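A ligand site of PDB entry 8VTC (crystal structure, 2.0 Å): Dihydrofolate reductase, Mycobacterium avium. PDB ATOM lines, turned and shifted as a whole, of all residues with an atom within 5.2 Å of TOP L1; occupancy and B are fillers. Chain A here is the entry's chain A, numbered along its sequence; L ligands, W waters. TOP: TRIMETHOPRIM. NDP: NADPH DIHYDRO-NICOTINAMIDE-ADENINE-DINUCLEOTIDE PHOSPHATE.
The side-chain carboxylate (OD2) of Asp 31 lies within hydrogen-bond range of a nitrogen (N2) of TOP L1 (2.7 Å).
The side-chain hydroxyl (OG) of Ser 53 is in hydrogen-bond range of an oxygen (O2D) of NDP L2.
N7 of TOP L1 sits at hydrogen-bond distance from O of Ile 102.
The side-chain hydroxyl (OG1) of Thr 50 is in hydrogen-bond range of an oxygen (O2A) of NDP L2, at 2.7 Å.
The backbone NH of Thr 50 is in hydrogen-bond range of an oxygen (O2A) of NDP L2.
The backbone carbonyl oxygen (O) of Val 9 sits at hydrogen-bond distance from a nitrogen (N7) of TOP L1 (2.8 Å).
N of Ala 11 sits at hydrogen-bond distance from O7N of NDP L2.
O of Ala 11 lies within hydrogen-bond range of N7N of NDP L2, 2.7 Å away.
The side-chain hydroxyl (OH) of Tyr 108 sits at hydrogen-bond distance from a nitrogen (N7) of TOP L1 (3.5 Å).
The backbone NH (N) of Val 9 lies within hydrogen-bond range of the backbone carbonyl oxygen (O) of Val 101, 3.0 Å away.
The side-chain hydroxyl (OG1) of Thr 121 is in hydrogen-bond range of the side-chain carboxylate (OD1) of Asp 31 (2.6 Å).
O of Ile 102 lies close to OH of Tyr 108.
The backbone carbonyl oxygen of Val 9 sits at hydrogen-bond distance from the side-chain hydroxyl of Tyr 108 (2.6 Å).
N of Gly 103 is in hydrogen-bond range of OH of Tyr 108.
N of Thr 121 is in hydrogen-bond range of O of Trp 10, 3.0 Å away.
Trp 10 touches TOP L1 (CA to N5, 3.3 Å).
Ala 11 touches TOP L1 (N to N4, 3.6 Å).
Ile 24 touches TOP L1 (CD1 to O19, 3.6 Å).
Leu 32 touches TOP L1 (CD2 to O13, 3.9 Å).
Phe 35 touches TOP L1.
Ser 53 touches TOP L1 (OG to C20, 3.4 Å).
Leu 54 touches TOP L1.
OG1 of Thr 121 touches N4 of TOP L1, 3.9 Å away.
Hydrophobic or aromatic side chains within 4 Å of TOP L1: Val 9, Ala 11, Ile 24, Leu 32, Phe 35, Leu 54 and Ile 102.
Of the 18 residues printed, 12 come within 4 Å of TOP L1.
Water W1 lies within hydrogen-bond range of OG1 of Thr 121 (2.8 Å), O of Trp 10 (3.3 Å) and N4 of TOP L1 (3.3 Å).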
ATOM      1  N   VAL A   9      -2.254 -18.032  24.880  1.00  0.00           N
ATOM      2  CA  VAL A   9      -0.938 -17.425  25.013  1.00  0.00           C
ATOM      3  C   VAL A   9      -0.586 -16.679  23.721  1.00  0.00           C
ATOM      4  O   VAL A   9      -0.723 -17.217  22.621  1.00  0.00           O
ATOM      5  CB  VAL A   9       0.103 -18.476  25.406  1.00  0.00           C
ATOM      6  CG1 VAL A   9       0.182 -19.590  24.371  1.00  0.00           C
ATOM      7  CG2 VAL A   9       1.476 -17.859  25.646  1.00  0.00           C
ATOM      8  N   TRP A  10      -0.106 -15.420  23.876  1.00  0.00           N
ATOM      9  CA  TRP A  10       0.333 -14.625  22.735  1.00  0.00           C
ATOM     10  C   TRP A  10       1.316 -13.530  23.153  1.00  0.00           C
ATOM     11  O   TRP A  10       1.465 -13.236  24.342  1.00  0.00           O
ATOM     12  CB  TRP A  10      -0.846 -13.970  22.002  1.00  0.00           C
ATOM     13  CG  TRP A  10      -1.514 -12.786  22.658  1.00  0.00           C
ATOM     14  CD1 TRP A  10      -1.198 -11.468  22.540  1.00  0.00           C
ATOM     15  CD2 TRP A  10      -2.684 -12.837  23.503  1.00  0.00           C
ATOM     16  NE1 TRP A  10      -2.090 -10.693  23.240  1.00  0.00           N
ATOM     17  CE2 TRP A  10      -3.020 -11.513  23.834  1.00  0.00           C
ATOM     18  CE3 TRP A  10      -3.488 -13.873  24.001  1.00  0.00           C
ATOM     19  CZ2 TRP A  10      -4.094 -11.197  24.648  1.00  0.00           C
ATOM     20  CZ3 TRP A  10      -4.557 -13.555  24.822  1.00  0.00           C
ATOM     21  CH2 TRP A  10      -4.874 -12.241  25.118  1.00  0.00           C
ATOM     22  N   ALA A  11       1.931 -12.943  22.115  1.00  0.00           N
ATOM     23  CA  ALA A  11       2.790 -11.785  22.206  1.00  0.00           C
ATOM     24  C   ALA A  11       2.211 -10.708  21.303  1.00  0.00           C
ATOM     25  O   ALA A  11       1.873 -10.978  20.140  1.00  0.00           O
ATOM     26  CB  ALA A  11       4.226 -12.114  21.803  1.00  0.00           C
ATOM     27  N   ILE A  24       5.675 -12.879  12.809  1.00  0.00           N
ATOM     28  CA  ILE A  24       5.723 -12.042  13.997  1.00  0.00           C
ATOM     29  C   ILE A  24       6.708 -10.913  13.724  1.00  0.00           C
ATOM     30  O   ILE A  24       7.834 -11.175  13.345  1.00  0.00           O
ATOM     31  CB  ILE A  24       6.126 -12.872  15.222  1.00  0.00           C
ATOM     32  CG1 ILE A  24       5.127 -14.029  15.425  1.00  0.00           C
ATOM     33  CG2 ILE A  24       6.265 -11.962  16.442  1.00  0.00           C
ATOM     34  CD1 ILE A  24       5.316 -14.822  16.690  1.00  0.00           C
ATOM     35  N   ASP A  31      10.723 -14.177  24.611  1.00  0.00           N
ATOM     36  CA  ASP A  31       9.312 -14.480  24.469  1.00  0.00           C
ATOM     37  C   ASP A  31       9.112 -15.935  24.045  1.00  0.00           C
ATOM     38  O   ASP A  31       8.192 -16.601  24.507  1.00  0.00           O
ATOM     39  CB  ASP A  31       8.595 -13.605  23.450  1.00  0.00           C
ATOM     40  CG  ASP A  31       7.181 -14.078  23.190  1.00  0.00           C
ATOM     41  OD1 ASP A  31       6.359 -13.969  24.141  1.00  0.00           O
ATOM     42  OD2 ASP A  31       6.931 -14.593  22.051  1.00  0.00           O
ATOM     43  N   LEU A  32       9.977 -16.399  23.138  1.00  0.00           N
ATOM     44  CA  LEU A  32       9.884 -17.778  22.708  1.00  0.00           C
ATOM     45  C   LEU A  32      10.202 -18.722  23.871  1.00  0.00           C
ATOM     46  O   LEU A  32       9.562 -19.770  23.985  1.00  0.00           O
ATOM     47  CB  LEU A  32      10.737 -18.043  21.477  1.00  0.00           C
ATOM     48  CG  LEU A  32      10.376 -17.168  20.274  1.00  0.00           C
ATOM     49  CD1 LEU A  32      11.214 -17.546  19.069  1.00  0.00           C
ATOM     50  CD2 LEU A  32       8.894 -17.226  19.911  1.00  0.00           C
ATOM     51  N   PHE A  35       7.159 -18.864  26.032  1.00  0.00           N
ATOM     52  CA  PHE A  35       6.144 -19.645  25.349  1.00  0.00           C
ATOM     53  C   PHE A  35       6.350 -21.147  25.585  1.00  0.00           C
ATOM     54  O   PHE A  35       5.424 -21.901  25.862  1.00  0.00           O
ATOM     55  CB  PHE A  35       6.179 -19.309  23.854  1.00  0.00           C
ATOM     56  CG  PHE A  35       5.333 -20.233  23.003  1.00  0.00           C
ATOM     57  CD1 PHE A  35       3.947 -20.126  23.017  1.00  0.00           C
ATOM     58  CD2 PHE A  35       5.917 -21.249  22.240  1.00  0.00           C
ATOM     59  CE1 PHE A  35       3.167 -20.977  22.250  1.00  0.00           C
ATOM     60  CE2 PHE A  35       5.126 -22.101  21.482  1.00  0.00           C
ATOM     61  CZ  PHE A  35       3.760 -21.971  21.488  1.00  0.00           C
ATOM     62  N   THR A  50      -1.477 -19.985  11.298  1.00  0.00           N
ATOM     63  CA  THR A  50      -0.378 -19.995  12.251  1.00  0.00           C
ATOM     64  C   THR A  50       0.511 -21.225  11.999  1.00  0.00           C
ATOM     65  O   THR A  50       1.745 -21.134  12.030  1.00  0.00           O
ATOM     66  CB  THR A  50      -0.927 -20.029  13.680  1.00  0.00           C
ATOM     67  OG1 THR A  50      -1.462 -18.746  13.997  1.00  0.00           O
ATOM     68  CG2 THR A  50       0.133 -20.380  14.694  1.00  0.00           C
ATOM     69  N   SER A  53       2.666 -20.370   9.287  1.00  0.00           N
ATOM     70  CA  SER A  53       3.642 -19.364   9.694  1.00  0.00           C
ATOM     71  C   SER A  53       4.887 -19.993  10.313  1.00  0.00           C
ATOM     72  O   SER A  53       5.992 -19.462  10.177  1.00  0.00           O
ATOM     73  CB  SER A  53       3.030 -18.409  10.677  1.00  0.00           C
ATOM     74  OG  SER A  53       3.895 -17.301  10.863  1.00  0.00           O
ATOM     75  N   LEU A  54       4.719 -21.094  11.045  1.00  0.00           N
ATOM     76  CA  LEU A  54       5.840 -21.756  11.696  1.00  0.00           C
ATOM     77  C   LEU A  54       6.760 -22.284  10.619  1.00  0.00           C
ATOM     78  O   LEU A  54       6.266 -22.899   9.672  1.00  0.00           O
ATOM     79  CB  LEU A  54       5.425 -22.937  12.567  1.00  0.00           C
ATOM     80  CG  LEU A  54       4.423 -22.640  13.658  1.00  0.00           C
ATOM     81  CD1 LEU A  54       3.899 -23.973  14.158  1.00  0.00           C
ATOM     82  CD2 LEU A  54       5.050 -21.828  14.787  1.00  0.00           C
ATOM     83  N   PRO A  55       8.095 -22.117  10.735  1.00  0.00           N
ATOM     84  CA  PRO A  55       9.037 -22.821   9.847  1.00  0.00           C
ATOM     85  C   PRO A  55       8.808 -24.329   9.926  1.00  0.00           C
ATOM     86  O   PRO A  55       8.543 -24.836  11.025  1.00  0.00           O
ATOM     87  CB  PRO A  55      10.410 -22.398  10.370  1.00  0.00           C
ATOM     88  CG  PRO A  55      10.151 -21.093  11.061  1.00  0.00           C
ATOM     89  CD  PRO A  55       8.790 -21.238  11.689  1.00  0.00           C
ATOM     90  N   VAL A  58      10.633 -26.431  12.449  1.00  0.00           N
ATOM     91  CA  VAL A  58      10.274 -26.169  13.823  1.00  0.00           C
ATOM     92  C   VAL A  58       8.955 -26.843  14.180  1.00  0.00           C
ATOM     93  O   VAL A  58       8.566 -26.857  15.344  1.00  0.00           O
ATOM     94  CB  VAL A  58      10.147 -24.646  14.024  1.00  0.00           C
ATOM     95  CG1 VAL A  58       9.653 -24.275  15.415  1.00  0.00           C
ATOM     96  CG2 VAL A  58      11.448 -23.918  13.704  1.00  0.00           C
ATOM     97  N   LEU A  61       5.459 -28.476  16.929  1.00  0.00           N
ATOM     98  CA  LEU A  61       6.176 -28.021  18.108  1.00  0.00           C
ATOM     99  C   LEU A  61       6.454 -29.204  19.022  1.00  0.00           C
ATOM    100  O   LEU A  61       5.509 -29.855  19.461  1.00  0.00           O
ATOM    101  CB  LEU A  61       5.362 -26.980  18.838  1.00  0.00           C
ATOM    102  CG  LEU A  61       5.100 -25.684  18.071  1.00  0.00           C
ATOM    103  CD1 LEU A  61       4.096 -24.850  18.822  1.00  0.00           C
ATOM    104  CD2 LEU A  61       6.399 -24.937  17.872  1.00  0.00           C
ATOM    105  N   VAL A 101      -4.189 -22.519  23.591  1.00  0.00           N
ATOM    106  CA  VAL A 101      -4.427 -21.943  22.276  1.00  0.00           C
ATOM    107  C   VAL A 101      -3.311 -20.934  22.004  1.00  0.00           C
ATOM    108  O   VAL A 101      -3.134 -20.007  22.796  1.00  0.00           O
ATOM    109  CB  VAL A 101      -5.816 -21.289  22.233  1.00  0.00           C
ATOM    110  CG1 VAL A 101      -6.061 -20.556  20.910  1.00  0.00           C
ATOM    111  CG2 VAL A 101      -6.899 -22.329  22.515  1.00  0.00           C
ATOM    112  N   ILE A 102      -2.618 -21.132  20.866  1.00  0.00           N
ATOM    113  CA  ILE A 102      -1.346 -20.489  20.576  1.00  0.00           C
ATOM    114  C   ILE A 102      -1.426 -19.595  19.322  1.00  0.00           C
ATOM    115  O   ILE A 102      -0.397 -19.154  18.814  1.00  0.00           O
ATOM    116  CB  ILE A 102      -0.212 -21.538  20.457  1.00  0.00           C
ATOM    117  CG1 ILE A 102      -0.302 -22.413  19.195  1.00  0.00           C
ATOM    118  CG2 ILE A 102      -0.143 -22.394  21.733  1.00  0.00           C
ATOM    119  CD1 ILE A 102       0.999 -23.112  18.839  1.00  0.00           C
ATOM    120  N   GLY A 103      -2.643 -19.336  18.848  1.00  0.00           N
ATOM    121  CA  GLY A 103      -2.868 -18.348  17.796  1.00  0.00           C
ATOM    122  C   GLY A 103      -3.508 -18.963  16.553  1.00  0.00           C
ATOM    123  O   GLY A 103      -3.655 -20.182  16.481  1.00  0.00           O
ATOM    124  N   TYR A 108      -8.020 -17.079  18.479  1.00  0.00           N
ATOM    125  CA  TYR A 108      -8.138 -16.498  19.819  1.00  0.00           C
ATOM    126  C   TYR A 108      -9.587 -16.067  20.058  1.00  0.00           C
ATOM    127  O   TYR A 108     -10.145 -16.309  21.135  1.00  0.00           O
ATOM    128  CB  TYR A 108      -7.176 -15.326  20.010  1.00  0.00           C
ATOM    129  CG  TYR A 108      -5.683 -15.644  20.085  1.00  0.00           C
ATOM    130  CD1 TYR A 108      -5.200 -16.650  20.914  1.00  0.00           C
ATOM    131  CD2 TYR A 108      -4.755 -14.907  19.339  1.00  0.00           C
ATOM    132  CE1 TYR A 108      -3.844 -16.945  20.966  1.00  0.00           C
ATOM    133  CE2 TYR A 108      -3.389 -15.184  19.406  1.00  0.00           C
ATOM    134  CZ  TYR A 108      -2.938 -16.212  20.212  1.00  0.00           C
ATOM    135  OH  TYR A 108      -1.613 -16.539  20.269  1.00  0.00           O
ATOM    136  N   THR A 121       2.749 -11.709  26.517  1.00  0.00           N
ATOM    137  CA  THR A 121       3.989 -10.953  26.468  1.00  0.00           C
ATOM    138  C   THR A 121       3.719  -9.646  25.729  1.00  0.00           C
ATOM    139  O   THR A 121       3.354  -9.695  24.568  1.00  0.00           O
ATOM    140  CB  THR A 121       5.087 -11.704  25.707  1.00  0.00           C
ATOM    141  OG1 THR A 121       5.229 -13.016  26.238  1.00  0.00           O
ATOM    142  CG2 THR A 121       6.390 -10.946  25.800  1.00  0.00           C
HETATM  143  C1  TOP L   1       4.743 -17.196  20.515  1.00  0.00           C
HETATM  144  N2  TOP L   1       4.890 -16.362  21.561  1.00  0.00           N
HETATM  145  C3  TOP L   1       3.860 -16.262  22.434  1.00  0.00           C
HETATM  146  N4  TOP L   1       4.033 -15.492  23.515  1.00  0.00           N
HETATM  147  N5  TOP L   1       2.674 -16.885  22.289  1.00  0.00           N
HETATM  148  C6  TOP L   1       2.526 -17.673  21.207  1.00  0.00           C
HETATM  149  N7  TOP L   1       1.334 -18.240  21.053  1.00  0.00           N
HETATM  150  C8  TOP L   1       3.571 -17.891  20.266  1.00  0.00           C
HETATM  151  C9  TOP L   1       3.397 -18.836  19.080  1.00  0.00           C
HETATM  152  C10 TOP L   1       4.553 -18.960  18.101  1.00  0.00           C
HETATM  153  C11 TOP L   1       5.708 -19.659  18.440  1.00  0.00           C
HETATM  154  C12 TOP L   1       6.761 -19.749  17.524  1.00  0.00           C
HETATM  155  O13 TOP L   1       7.967 -20.341  17.728  1.00  0.00           O
HETATM  156  C14 TOP L   1       8.169 -21.053  18.939  1.00  0.00           C
HETATM  157  C15 TOP L   1       6.711 -19.052  16.323  1.00  0.00           C
HETATM  158  O16 TOP L   1       7.779 -19.215  15.477  1.00  0.00           O
HETATM  159  C17 TOP L   1       8.410 -18.002  15.092  1.00  0.00           C
HETATM  160  C18 TOP L   1       5.526 -18.397  15.953  1.00  0.00           C
HETATM  161  O19 TOP L   1       5.526 -17.814  14.721  1.00  0.00           O
HETATM  162  C20 TOP L   1       4.294 -17.347  14.206  1.00  0.00           C
HETATM  163  C21 TOP L   1       4.473 -18.346  16.854  1.00  0.00           C
HETATM  164  PA  NDP L   2      -5.169 -18.048  12.297  1.00  0.00           P
HETATM  165  O1A NDP L   2      -6.087 -17.586  13.364  1.00  0.00           O
HETATM  166  O2A NDP L   2      -3.857 -18.651  12.666  1.00  0.00           O
HETATM  167  O5B NDP L   2      -5.879 -19.091  11.318  1.00  0.00           O
HETATM  168  C5B NDP L   2      -7.056 -18.738  10.583  1.00  0.00           C
HETATM  169  C4B NDP L   2      -7.565 -19.992   9.938  1.00  0.00           C
HETATM  170  O4B NDP L   2      -8.204 -20.819  10.940  1.00  0.00           O
HETATM  171  C3B NDP L   2      -8.614 -19.826   8.838  1.00  0.00           C
HETATM  172  O3B NDP L   2      -7.974 -19.488   7.619  1.00  0.00           O
HETATM  173  C2B NDP L   2      -9.194 -21.227   8.823  1.00  0.00           C
HETATM  174  O2B NDP L   2      -8.339 -22.177   8.178  1.00  0.00           O
HETATM  175  C1B NDP L   2      -9.229 -21.563  10.317  1.00  0.00           C
HETATM  176  N9A NDP L   2     -10.474 -21.188  10.949  1.00  0.00           N
HETATM  177  C8A NDP L   2     -10.876 -19.946  11.358  1.00  0.00           C
HETATM  178  N7A NDP L   2     -12.058 -19.935  11.924  1.00  0.00           N
HETATM  179  C5A NDP L   2     -12.448 -21.267  11.873  1.00  0.00           C
HETATM  180  C6A NDP L   2     -13.602 -21.921  12.320  1.00  0.00           C
HETATM  181  N6A NDP L   2     -14.615 -21.293  12.917  1.00  0.00           N
HETATM  182  N1A NDP L   2     -13.665 -23.257  12.132  1.00  0.00           N
HETATM  183  C2A NDP L   2     -12.634 -23.888  11.548  1.00  0.00           C
HETATM  184  N3A NDP L   2     -11.497 -23.381  11.099  1.00  0.00           N
HETATM  185  C4A NDP L   2     -11.473 -22.056  11.292  1.00  0.00           C
HETATM  186  O3  NDP L   2      -4.913 -16.810  11.310  1.00  0.00           O
HETATM  187  PN  NDP L   2      -4.613 -15.265  11.545  1.00  0.00           P
HETATM  188  O1N NDP L   2      -5.787 -14.702  12.268  1.00  0.00           O
HETATM  189  O2N NDP L   2      -4.255 -14.713  10.209  1.00  0.00           O
HETATM  190  O5D NDP L   2      -3.322 -15.217  12.489  1.00  0.00           O
HETATM  191  C5D NDP L   2      -2.030 -15.647  11.925  1.00  0.00           C
HETATM  192  C4D NDP L   2      -1.000 -14.559  12.126  1.00  0.00           C
HETATM  193  O4D NDP L   2      -0.767 -14.427  13.544  1.00  0.00           O
HETATM  194  C3D NDP L   2       0.381 -14.772  11.496  1.00  0.00           C
HETATM  195  O3D NDP L   2       0.947 -13.546  11.067  1.00  0.00           O
HETATM  196  C2D NDP L   2       1.189 -15.346  12.665  1.00  0.00           C
HETATM  197  O2D NDP L   2       2.592 -15.161  12.481  1.00  0.00           O
HETATM  198  C1D NDP L   2       0.618 -14.531  13.827  1.00  0.00           C
HETATM  199  N1N NDP L   2       0.804 -15.158  15.178  1.00  0.00           N
HETATM  200  C2N NDP L   2       1.400 -14.422  16.174  1.00  0.00           C
HETATM  201  C3N NDP L   2       1.482 -14.863  17.464  1.00  0.00           C
HETATM  202  C7N NDP L   2       1.982 -13.961  18.535  1.00  0.00           C
HETATM  203  O7N NDP L   2       1.819 -14.351  19.696  1.00  0.00           O
HETATM  204  N7N NDP L   2       2.610 -12.816  18.268  1.00  0.00           N
HETATM  205  C4N NDP L   2       1.082 -16.260  17.782  1.00  0.00           C
HETATM  206  C5N NDP L   2       0.578 -17.026  16.619  1.00  0.00           C
HETATM  207  C6N NDP L   2       0.428 -16.462  15.433  1.00  0.00           C
HETATM  208  P2B NDP L   2      -8.888 -22.721   6.769  1.00  0.00           P
HETATM  209  O1X NDP L   2      -8.827 -21.498   5.884  1.00  0.00           O
HETATM  210  O2X NDP L   2      -7.879 -23.786   6.369  1.00  0.00           O
HETATM  211  O3X NDP L   2     -10.276 -23.262   6.967  1.00  0.00           O
HETATM  212  O   HOH W   1       3.168 -14.814  26.624  1.00  0.00           O
HETATM  213  O   HOH W   2       8.026 -23.514  21.347  1.00  0.00           O
HETATM  214  O   HOH W   3       9.492 -21.328  21.910  1.00  0.00           O
